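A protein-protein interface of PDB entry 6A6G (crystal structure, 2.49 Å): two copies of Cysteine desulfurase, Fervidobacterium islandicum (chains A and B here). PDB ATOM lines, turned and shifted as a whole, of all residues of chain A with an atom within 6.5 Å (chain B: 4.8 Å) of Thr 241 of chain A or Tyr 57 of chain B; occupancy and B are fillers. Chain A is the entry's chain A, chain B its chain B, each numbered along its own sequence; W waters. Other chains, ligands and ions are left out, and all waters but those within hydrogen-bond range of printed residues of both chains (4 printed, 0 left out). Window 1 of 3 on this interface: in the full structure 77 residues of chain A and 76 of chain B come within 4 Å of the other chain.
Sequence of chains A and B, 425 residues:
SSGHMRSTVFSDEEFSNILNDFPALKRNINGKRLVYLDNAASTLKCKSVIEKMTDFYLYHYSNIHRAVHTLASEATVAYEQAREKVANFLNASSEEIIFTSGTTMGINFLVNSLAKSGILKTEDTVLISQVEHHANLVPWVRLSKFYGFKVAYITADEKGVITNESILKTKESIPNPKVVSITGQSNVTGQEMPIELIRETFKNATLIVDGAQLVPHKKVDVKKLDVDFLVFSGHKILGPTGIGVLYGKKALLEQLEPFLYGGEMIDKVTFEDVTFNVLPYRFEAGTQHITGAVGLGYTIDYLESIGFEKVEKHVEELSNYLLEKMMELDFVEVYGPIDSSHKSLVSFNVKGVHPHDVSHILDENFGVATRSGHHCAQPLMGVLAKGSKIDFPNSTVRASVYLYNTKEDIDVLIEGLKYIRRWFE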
ATOM      1  N   ALA A  24      14.664 -27.942  38.442  1.00  0.00           N
ATOM      2  CA  ALA A  24      16.054 -27.853  37.981  1.00  0.00           C
ATOM      3  C   ALA A  24      17.012 -28.192  39.107  1.00  0.00           C
ATOM      4  O   ALA A  24      18.062 -28.777  38.879  1.00  0.00           O
ATOM      5  CB  ALA A  24      16.346 -26.485  37.435  1.00  0.00           C
ATOM      6  N   SER A  42      19.919 -15.123  34.264  1.00  0.00           N
ATOM      7  CA  SER A  42      18.548 -15.619  34.167  1.00  0.00           C
ATOM      8  C   SER A  42      18.286 -16.565  35.320  1.00  0.00           C
ATOM      9  O   SER A  42      19.200 -17.086  35.937  1.00  0.00           O
ATOM     10  CB  SER A  42      18.292 -16.354  32.837  1.00  0.00           C
ATOM     11  OG  SER A  42      16.942 -16.237  32.475  1.00  0.00           O
ATOM     12  N   THR A  43      17.017 -16.823  35.562  1.00  0.00           N
ATOM     13  CA  THR A  43      16.616 -17.532  36.731  1.00  0.00           C
ATOM     14  C   THR A  43      15.909 -18.798  36.329  1.00  0.00           C
ATOM     15  O   THR A  43      15.340 -18.888  35.263  1.00  0.00           O
ATOM     16  CB  THR A  43      15.747 -16.623  37.630  1.00  0.00           C
ATOM     17  OG1 THR A  43      14.636 -16.112  36.900  1.00  0.00           O
ATOM     18  CG2 THR A  43      16.536 -15.467  38.028  1.00  0.00           C
ATOM     19  N   LEU A  44      15.948 -19.774  37.213  1.00  0.00           N
ATOM     20  CA  LEU A  44      15.241 -21.035  37.045  1.00  0.00           C
ATOM     21  C   LEU A  44      13.745 -20.791  37.170  1.00  0.00           C
ATOM     22  O   LEU A  44      13.323 -19.804  37.764  1.00  0.00           O
ATOM     23  CB  LEU A  44      15.713 -22.022  38.133  1.00  0.00           C
ATOM     24  CG  LEU A  44      17.241 -22.195  38.233  1.00  0.00           C
ATOM     25  CD1 LEU A  44      17.574 -22.982  39.481  1.00  0.00           C
ATOM     26  CD2 LEU A  44      17.822 -22.864  36.994  1.00  0.00           C
ATOM     27  N   LYS A  45      12.946 -21.701  36.644  1.00  0.00           N
ATOM     28  CA  LYS A  45      11.512 -21.526  36.623  1.00  0.00           C
ATOM     29  C   LYS A  45      10.796 -22.429  37.590  1.00  0.00           C
ATOM     30  O   LYS A  45      11.178 -23.580  37.831  1.00  0.00           O
ATOM     31  CB  LYS A  45      10.957 -21.790  35.209  1.00  0.00           C
ATOM     32  CG  LYS A  45      11.740 -21.136  34.072  1.00  0.00           C
ATOM     33  CD  LYS A  45      11.880 -19.638  34.268  1.00  0.00           C
ATOM     34  CE  LYS A  45      12.700 -19.038  33.174  1.00  0.00           C
ATOM     35  NZ  LYS A  45      13.399 -17.860  33.734  1.00  0.00           N
ATOM     36  N   ILE A  50       4.749 -22.547  35.434  1.00  0.00           N
ATOM     37  CA  ILE A  50       4.763 -23.177  34.117  1.00  0.00           C
ATOM     38  C   ILE A  50       3.506 -24.011  33.873  1.00  0.00           C
ATOM     39  O   ILE A  50       2.989 -24.033  32.770  1.00  0.00           O
ATOM     40  CB  ILE A  50       5.999 -24.090  33.959  1.00  0.00           C
ATOM     41  CG1 ILE A  50       7.307 -23.302  34.082  1.00  0.00           C
ATOM     42  CG2 ILE A  50       5.968 -24.837  32.636  1.00  0.00           C
ATOM     43  CD1 ILE A  50       7.507 -22.221  33.043  1.00  0.00           C
ATOM     44  N   MET A  53       0.899 -21.821  32.651  1.00  0.00           N
ATOM     45  CA  MET A  53       1.099 -21.380  31.282  1.00  0.00           C
ATOM     46  C   MET A  53       0.666 -22.476  30.315  1.00  0.00           C
ATOM     47  O   MET A  53       0.177 -22.208  29.208  1.00  0.00           O
ATOM     48  CB  MET A  53       2.564 -21.051  31.023  1.00  0.00           C
ATOM     49  CG  MET A  53       3.099 -19.771  31.658  1.00  0.00           C
ATOM     50  SD  MET A  53       4.898 -19.567  31.426  1.00  0.00           S
ATOM     51  CE  MET A  53       4.942 -19.109  29.694  1.00  0.00           C
ATOM     52  N   SER A 101       9.618  -7.316  24.532  1.00  0.00           N
ATOM     53  CA  SER A 101      10.293  -8.610  24.469  1.00  0.00           C
ATOM     54  C   SER A 101      11.414  -8.728  25.513  1.00  0.00           C
ATOM     55  O   SER A 101      11.982  -9.826  25.697  1.00  0.00           O
ATOM     56  CB  SER A 101      10.898  -8.807  23.075  1.00  0.00           C
ATOM     57  OG  SER A 101      11.907  -7.861  22.865  1.00  0.00           O
ATOM     58  N   GLY A 234      11.240 -10.261  32.214  1.00  0.00           N
ATOM     59  CA  GLY A 234      10.602 -11.319  32.962  1.00  0.00           C
ATOM     60  C   GLY A 234      11.507 -12.488  33.274  1.00  0.00           C
ATOM     61  O   GLY A 234      11.325 -13.159  34.268  1.00  0.00           O
ATOM     62  N   HIS A 235      12.481 -12.785  32.430  1.00  0.00           N
ATOM     63  CA  HIS A 235      13.189 -14.039  32.652  1.00  0.00           C
ATOM     64  C   HIS A 235      14.117 -13.944  33.853  1.00  0.00           C
ATOM     65  O   HIS A 235      14.559 -14.955  34.369  1.00  0.00           O
ATOM     66  CB  HIS A 235      13.931 -14.506  31.404  1.00  0.00           C
ATOM     67  CG  HIS A 235      15.028 -13.594  30.992  1.00  0.00           C
ATOM     68  ND1 HIS A 235      16.328 -13.795  31.381  1.00  0.00           N
ATOM     69  CD2 HIS A 235      15.018 -12.467  30.234  1.00  0.00           C
ATOM     70  CE1 HIS A 235      17.073 -12.821  30.879  1.00  0.00           C
ATOM     71  NE2 HIS A 235      16.304 -12.010  30.171  1.00  0.00           N
ATOM     72  N   GLY A 239      10.282 -15.513  35.497  1.00  0.00           N
ATOM     73  CA  GLY A 239       9.249 -15.523  34.462  1.00  0.00           C
ATOM     74  C   GLY A 239       9.676 -16.141  33.143  1.00  0.00           C
ATOM     75  O   GLY A 239      10.818 -16.562  32.990  1.00  0.00           O
ATOM     76  N   PRO A 240       8.762 -16.165  32.167  1.00  0.00           N
ATOM     77  CA  PRO A 240       9.043 -16.697  30.838  1.00  0.00           C
ATOM     78  C   PRO A 240      10.093 -15.878  30.120  1.00  0.00           C
ATOM     79  O   PRO A 240      10.314 -14.692  30.482  1.00  0.00           O
ATOM     80  CB  PRO A 240       7.698 -16.544  30.115  1.00  0.00           C
ATOM     81  CG  PRO A 240       6.693 -16.404  31.199  1.00  0.00           C
ATOM     82  CD  PRO A 240       7.403 -15.608  32.228  1.00  0.00           C
ATOM     83  N   THR A 241      10.720 -16.478  29.109  1.00  0.00           N
ATOM     84  CA  THR A 241      11.554 -15.686  28.221  1.00  0.00           C
ATOM     85  C   THR A 241      10.671 -14.961  27.227  1.00  0.00           C
ATOM     86  O   THR A 241       9.470 -15.241  27.102  1.00  0.00           O
ATOM     87  CB  THR A 241      12.602 -16.515  27.455  1.00  0.00           C
ATOM     88  OG1 THR A 241      11.976 -17.555  26.730  1.00  0.00           O
ATOM     89  CG2 THR A 241      13.650 -17.095  28.422  1.00  0.00           C
ATOM     90  N   GLY A 242      11.286 -14.011  26.539  1.00  0.00           N
ATOM     91  CA  GLY A 242      10.623 -13.275  25.455  1.00  0.00           C
ATOM     92  C   GLY A 242       9.638 -12.212  25.916  1.00  0.00           C
ATOM     93  O   GLY A 242       8.900 -11.646  25.095  1.00  0.00           O
ATOM     94  N   ILE A 243       9.637 -11.920  27.216  1.00  0.00           N
ATOM     95  CA  ILE A 243       8.720 -10.913  27.762  1.00  0.00           C
ATOM     96  C   ILE A 243       9.444  -9.873  28.628  1.00  0.00           C
ATOM     97  O   ILE A 243      10.268 -10.214  29.477  1.00  0.00           O
ATOM     98  CB  ILE A 243       7.563 -11.604  28.534  1.00  0.00           C
ATOM     99  CG1 ILE A 243       6.461 -10.597  28.886  1.00  0.00           C
ATOM    100  CG2 ILE A 243       8.080 -12.310  29.759  1.00  0.00           C
ATOM    101  CD1 ILE A 243       5.739 -10.087  27.673  1.00  0.00           C
ATOM    102  N   HIS A 289       3.796 -11.271  23.086  1.00  0.00           N
ATOM    103  CA  HIS A 289       3.978 -12.501  23.815  1.00  0.00           C
ATOM    104  C   HIS A 289       2.865 -12.717  24.869  1.00  0.00           C
ATOM    105  O   HIS A 289       3.109 -12.634  26.069  1.00  0.00           O
ATOM    106  CB  HIS A 289       5.388 -12.598  24.486  1.00  0.00           C
ATOM    107  CG  HIS A 289       5.716 -13.989  24.955  1.00  0.00           C
ATOM    108  ND1 HIS A 289       4.939 -15.083  24.624  1.00  0.00           N
ATOM    109  CD2 HIS A 289       6.749 -14.469  25.691  1.00  0.00           C
ATOM    110  CE1 HIS A 289       5.475 -16.172  25.156  1.00  0.00           C
ATOM    111  NE2 HIS A 289       6.561 -15.825  25.825  1.00  0.00           N
ATOM    112  N   GLY A 292       3.493 -15.134  27.506  1.00  0.00           N
ATOM    113  CA  GLY A 292       4.559 -14.600  28.316  1.00  0.00           C
ATOM    114  C   GLY A 292       4.062 -13.582  29.315  1.00  0.00           C
ATOM    115  O   GLY A 292       4.475 -13.591  30.454  1.00  0.00           O
ATOM    116  N   MET B  53       8.330 -28.015  25.564  1.00  0.00           N
ATOM    117  CA  MET B  53       8.611 -26.647  25.993  1.00  0.00           C
ATOM    118  C   MET B  53       8.654 -26.560  27.513  1.00  0.00           C
ATOM    119  O   MET B  53       9.506 -25.898  28.055  1.00  0.00           O
ATOM    120  CB  MET B  53       7.566 -25.653  25.503  1.00  0.00           C
ATOM    121  CG  MET B  53       7.588 -25.298  24.023  1.00  0.00           C
ATOM    122  SD  MET B  53       6.317 -24.036  23.650  1.00  0.00           S
ATOM    123  CE  MET B  53       6.982 -22.663  24.594  1.00  0.00           C
ATOM    124  N   THR B  54       7.738 -27.212  28.217  1.00  0.00           N
ATOM    125  CA  THR B  54       7.765 -27.041  29.651  1.00  0.00           C
ATOM    126  C   THR B  54       8.912 -27.848  30.208  1.00  0.00           C
ATOM    127  O   THR B  54       9.534 -27.428  31.167  1.00  0.00           O
ATOM    128  CB  THR B  54       6.434 -27.378  30.354  1.00  0.00           C
ATOM    129  OG1 THR B  54       6.118 -28.750  30.183  1.00  0.00           O
ATOM    130  CG2 THR B  54       5.339 -26.563  29.808  1.00  0.00           C
ATOM    131  N   ASP B  55       9.213 -28.990  29.594  1.00  0.00           N
ATOM    132  CA  ASP B  55      10.392 -29.778  29.985  1.00  0.00           C
ATOM    133  C   ASP B  55      11.673 -28.920  29.894  1.00  0.00           C
ATOM    134  O   ASP B  55      12.536 -28.959  30.745  1.00  0.00           O
ATOM    135  CB  ASP B  55      10.505 -31.046  29.136  1.00  0.00           C
ATOM    136  CG  ASP B  55      11.737 -31.888  29.470  1.00  0.00           C
ATOM    137  OD1 ASP B  55      11.674 -32.601  30.489  1.00  0.00           O
ATOM    138  OD2 ASP B  55      12.747 -31.878  28.698  1.00  0.00           O
ATOM    139  N   PHE B  56      11.741 -28.098  28.872  1.00  0.00           N
ATOM    140  CA  PHE B  56      12.904 -27.298  28.655  1.00  0.00           C
ATOM    141  C   PHE B  56      13.023 -26.256  29.745  1.00  0.00           C
ATOM    142  O   PHE B  56      14.089 -26.110  30.335  1.00  0.00           O
ATOM    143  CB  PHE B  56      12.842 -26.665  27.288  1.00  0.00           C
ATOM    144  CG  PHE B  56      14.007 -25.811  26.991  1.00  0.00           C
ATOM    145  CD1 PHE B  56      15.180 -26.358  26.554  1.00  0.00           C
ATOM    146  CD2 PHE B  56      13.935 -24.460  27.151  1.00  0.00           C
ATOM    147  CE1 PHE B  56      16.280 -25.575  26.259  1.00  0.00           C
ATOM    148  CE2 PHE B  56      15.023 -23.667  26.840  1.00  0.00           C
ATOM    149  CZ  PHE B  56      16.212 -24.232  26.407  1.00  0.00           C
ATOM    150  N   TYR B  57      11.926 -25.557  30.015  1.00  0.00           N
ATOM    151  CA  TYR B  57      11.899 -24.512  31.026  1.00  0.00           C
ATOM    152  C   TYR B  57      12.310 -25.049  32.374  1.00  0.00           C
ATOM    153  O   TYR B  57      13.083 -24.419  33.083  1.00  0.00           O
ATOM    154  CB  TYR B  57      10.489 -23.904  31.174  1.00  0.00           C
ATOM    155  CG  TYR B  57      10.206 -22.608  30.418  1.00  0.00           C
ATOM    156  CD1 TYR B  57      11.126 -21.561  30.415  1.00  0.00           C
ATOM    157  CD2 TYR B  57       8.988 -22.415  29.764  1.00  0.00           C
ATOM    158  CE1 TYR B  57      10.870 -20.388  29.748  1.00  0.00           C
ATOM    159  CE2 TYR B  57       8.719 -21.249  29.106  1.00  0.00           C
ATOM    160  CZ  TYR B  57       9.658 -20.233  29.104  1.00  0.00           C
ATOM    161  OH  TYR B  57       9.396 -19.063  28.441  1.00  0.00           O
ATOM    162  N   LEU B  58      11.765 -26.189  32.748  1.00  0.00           N
ATOM    163  CA  LEU B  58      12.021 -26.732  34.073  1.00  0.00           C
ATOM    164  C   LEU B  58      13.368 -27.475  34.249  1.00  0.00           C
ATOM    165  O   LEU B  58      13.892 -27.528  35.356  1.00  0.00           O
ATOM    166  CB  LEU B  58      10.871 -27.634  34.505  1.00  0.00           C
ATOM    167  CG  LEU B  58       9.503 -26.964  34.601  1.00  0.00           C
ATOM    168  CD1 LEU B  58       8.431 -27.974  34.938  1.00  0.00           C
ATOM    169  CD2 LEU B  58       9.543 -25.838  35.637  1.00  0.00           C
ATOM    170  N   TYR B  59      13.946 -28.022  33.191  1.00  0.00           N
ATOM    171  CA  TYR B  59      15.103 -28.904  33.380  1.00  0.00           C
ATOM    172  C   TYR B  59      16.370 -28.547  32.622  1.00  0.00           C
ATOM    173  O   TYR B  59      17.442 -28.917  33.062  1.00  0.00           O
ATOM    174  CB  TYR B  59      14.711 -30.365  33.055  1.00  0.00           C
ATOM    175  CG  TYR B  59      13.724 -30.957  34.023  1.00  0.00           C
ATOM    176  CD1 TYR B  59      14.140 -31.494  35.242  1.00  0.00           C
ATOM    177  CD2 TYR B  59      12.372 -30.988  33.723  1.00  0.00           C
ATOM    178  CE1 TYR B  59      13.231 -32.058  36.135  1.00  0.00           C
ATOM    179  CE2 TYR B  59      11.455 -31.543  34.605  1.00  0.00           C
ATOM    180  CZ  TYR B  59      11.893 -32.069  35.800  1.00  0.00           C
ATOM    181  OH  TYR B  59      10.964 -32.559  36.678  1.00  0.00           O
ATOM    182  N   TYR B  61      17.004 -25.220  31.202  1.00  0.00           N
ATOM    183  CA  TYR B  61      16.894 -23.806  30.884  1.00  0.00           C
ATOM    184  C   TYR B  61      18.032 -23.005  31.460  1.00  0.00           C
ATOM    185  O   TYR B  61      18.426 -23.232  32.598  1.00  0.00           O
ATOM    186  CB  TYR B  61      15.613 -23.228  31.465  1.00  0.00           C
ATOM    187  CG  TYR B  61      15.612 -21.742  31.307  1.00  0.00           C
ATOM    188  CD1 TYR B  61      15.363 -21.201  30.081  1.00  0.00           C
ATOM    189  CD2 TYR B  61      15.974 -20.902  32.345  1.00  0.00           C
ATOM    190  CE1 TYR B  61      15.440 -19.860  29.884  1.00  0.00           C
ATOM    191  CE2 TYR B  61      16.035 -19.542  32.151  1.00  0.00           C
ATOM    192  CZ  TYR B  61      15.760 -19.034  30.908  1.00  0.00           C
ATOM    193  OH  TYR B  61      15.795 -17.699  30.619  1.00  0.00           O
ATOM    194  N   GLN B 288      16.972 -13.425  23.722  1.00  0.00           N
ATOM    195  CA  GLN B 288      15.856 -13.709  22.847  1.00  0.00           C
ATOM    196  C   GLN B 288      14.787 -14.549  23.570  1.00  0.00           C
ATOM    197  O   GLN B 288      14.988 -14.994  24.721  1.00  0.00           O
ATOM    198  CB  GLN B 288      16.403 -14.438  21.612  1.00  0.00           C
ATOM    199  CG  GLN B 288      17.367 -13.589  20.790  1.00  0.00           C
ATOM    200  CD  GLN B 288      16.710 -12.269  20.387  1.00  0.00           C
ATOM    201  OE1 GLN B 288      15.721 -12.262  19.637  1.00  0.00           O
ATOM    202  NE2 GLN B 288      17.237 -11.143  20.909  1.00  0.00           N
ATOM    203  N   HIS B 289      13.660 -14.776  22.905  1.00  0.00           N
ATOM    204  CA  HIS B 289      12.699 -15.736  23.389  1.00  0.00           C
ATOM    205  C   HIS B 289      13.278 -17.164  23.238  1.00  0.00           C
ATOM    206  O   HIS B 289      12.989 -17.909  22.251  1.00  0.00           O
ATOM    207  CB  HIS B 289      11.373 -15.565  22.665  1.00  0.00           C
ATOM    208  CG  HIS B 289      10.258 -16.338  23.295  1.00  0.00           C
ATOM    209  ND1 HIS B 289      10.412 -17.018  24.487  1.00  0.00           N
ATOM    210  CD2 HIS B 289       8.962 -16.500  22.931  1.00  0.00           C
ATOM    211  CE1 HIS B 289       9.265 -17.602  24.804  1.00  0.00           C
ATOM    212  NE2 HIS B 289       8.374 -17.306  23.874  1.00  0.00           N
ATOM    213  N   ILE B 290      14.106 -17.545  24.215  1.00  0.00           N
ATOM    214  CA  ILE B 290      14.857 -18.780  24.085  1.00  0.00           C
ATOM    215  C   ILE B 290      13.916 -19.972  23.978  1.00  0.00           C
ATOM    216  O   ILE B 290      14.025 -20.756  23.076  1.00  0.00           O
ATOM    217  CB  ILE B 290      15.804 -18.990  25.245  1.00  0.00           C
ATOM    218  CG1 ILE B 290      16.909 -17.932  25.208  1.00  0.00           C
ATOM    219  CG2 ILE B 290      16.415 -20.376  25.161  1.00  0.00           C
ATOM    220  CD1 ILE B 290      17.560 -17.649  26.558  1.00  0.00           C
ATOM    221  N   THR B 291      12.965 -20.060  24.889  1.00  0.00           N
ATOM    222  CA  THR B 291      12.072 -21.212  24.972  1.00  0.00           C
ATOM    223  C   THR B 291      11.075 -21.194  23.812  1.00  0.00           C
ATOM    224  O   THR B 291      10.630 -22.231  23.355  1.00  0.00           O
ATOM    225  CB  THR B 291      11.277 -21.233  26.287  1.00  0.00           C
ATOM    226  OG1 THR B 291      12.170 -21.227  27.407  1.00  0.00           O
ATOM    227  CG2 THR B 291      10.465 -22.491  26.356  1.00  0.00           C
ATOM    228  N   GLY B 292      10.764 -20.004  23.323  1.00  0.00           N
ATOM    229  CA  GLY B 292       9.927 -19.889  22.162  1.00  0.00           C
ATOM    230  C   GLY B 292      10.554 -20.449  20.897  1.00  0.00           C
ATOM    231  O   GLY B 292       9.876 -21.093  20.108  1.00  0.00           O
HETATM  232  O   HOH W   1       7.026 -18.142  27.237  1.00  0.00           O
HETATM  233  O   HOH W   2      13.522 -25.200  37.825  1.00  0.00           O
HETATM  234  O   HOH W   3      13.847 -13.535  27.042  1.00  0.00           O
HETATM  235  O   HOH W   4      14.351 -24.026  35.383  1.00  0.00           O
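His 289 of chain B touches its own counterpart, His 289 of chain A. Positions printed for both chains: 53, 289 and 292. Of the 19 pairs that touch across the chains among the printed residues, 1 has its exchanged pair printed and touching as well.
Hydrophobic or aromatic side chains of chain B that line the printed part of chain A: Tyr 57, Leu 58, Tyr 61 and His 289. Of the 17 printed residues of chain A, 10 touch a printed residue of chain B. Among the printed residues, 19 pairs touch across the chains. Among the printed residues, no Asp or Glu carboxylate lies within 4 Å of a Lys or Arg side-chain nitrogen of the other chain.
O of Tyr 57 of chain B touches CG of Lys 45 of chain A (3.7 Å). Leu 58 of chain B touches Lys 45 of chain A. Tyr 61 of chain B touches Lys 45 of chain A. CG2 of Ile 50 of chain A touches CG2 of Thr 54 of chain B (3.4 Å). CD1 of Ile 50 of chain A touches CD2 of Tyr 57 of chain B, 3.6 Å away. CG1 of Ile 50 of chain A touches CD2 of Leu 58 of chain B, 3.7 Å away. Tyr 57 of chain B touches Pro 240 of chain A. Tyr 61 of chain B touches Thr 241 of chain A. CB of Thr 241 of chain A touches O of Gln 288 of chain B, 3.9 Å away. CB of His 289 of chain B touches CA of Gly 242 of chain A, at 3.7 Å.
O of Leu 58 of chain B sits at hydrogen-bond distance from N of Ala 24 of chain A (3.2 Å). The side-chain hydroxyl (OG) of Ser 42 of chain A is in hydrogen-bond range of the side-chain hydroxyl (OH) of Tyr 61 of chain B (2.6 Å). The backbone NH of Thr 241 of chain A lies within hydrogen-bond range of the side-chain hydroxyl of Tyr 57 of chain B, 3.0 Å away. ND1 of His 289 of chain B is in hydrogen-bond range of OG1 of Thr 241 of chain A (2.8 Å). The side-chain hydroxyl of Thr 241 of chain A lies within hydrogen-bond range of the backbone NH of Ile 290 of chain B, at 3.3 Å. OG1 of Thr 241 of chain A sits at hydrogen-bond distance from N of Thr 291 of chain B. A ring nitrogen (NE2) of His 289 of chain B sits at hydrogen-bond distance from a ring nitrogen (NE2) of His 289 of chain A.
ND1 of His 235 of chain A lies within hydrogen-bond range of OG of Ser 42 of chain A, at 2.7 Å. OG1 of Thr 43 of chain A sits at hydrogen-bond distance from O of His 235 of chain A (2.8 Å). O of Pro 240 of chain A sits at hydrogen-bond distance from N of His 235 of chain A, 3.5 Å away. N of Gly 292 of chain A is in hydrogen-bond range of ND1 of His 289 of chain A, 3.2 Å away. O of Phe 56 of chain B lies within hydrogen-bond range of N of Tyr 61 of chain B. ND1 of His 289 of chain B lies close to N of Gly 292 of chain B (3.2 Å).
Water W3 bridges N of Gly 242 of chain A (2.7 Å) and O of Gln 288 of chain B (3.0 Å). Water W4 bridges the backbone carbonyl oxygen of Tyr 57 of chain B (2.7 Å) and the backbone NH of Lys 45 of chain A (3.0 Å). Water W1 bridges a ring nitrogen (NE2) of His 289 of chain A (2.8 Å) and the side-chain hydroxyl (OH) of Tyr 57 of chain B (2.8 Å). Water W2 lies within hydrogen-bond range of O of Lys 45 of chain A (2.8 Å), N of Ala 24 of chain A (3.0 Å) and O of Leu 58 of chain B (3.4 Å).
Thr 241 of chain A touches six residues of chain B. Of chain A, only Lys 45, Ile 50, Pro 240 and Thr 241 come within 4 Å of Tyr 57 of chain B. Printed residues of chain B within 4 Å of His 289 of chain A: His 289 (3.0 Å). Printed residues of chain B within 4 Å of Ala 24 of chain A: Leu 58. Of the printed residues of chain A, Tyr 61 of chain B touches Ser 42, Thr 43, Lys 45, His 235 and Thr 241. Printed residues of chain A within 4 Å of Leu 58 of chain B: Ala 24 (3.2 Å), Lys 45 (3.5 Å) and Ile 50 (3.7 Å). Met 53 of chain A touches none of the printed residues of chain B. Gly 239 of chain A touches none of the printed residues of chain B. The nearest residue of chain B that does not touch Thr 241 of chain A is Gly 292 of chain B (4.4 Å). The nearest residue of chain A that does not touch Tyr 57 of chain B is Met 53 of chain A (4.4 Å). The nearest printed residue of chain A that does not touch Gln 288 of chain B is Gly 242 of chain A (4.2 Å).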
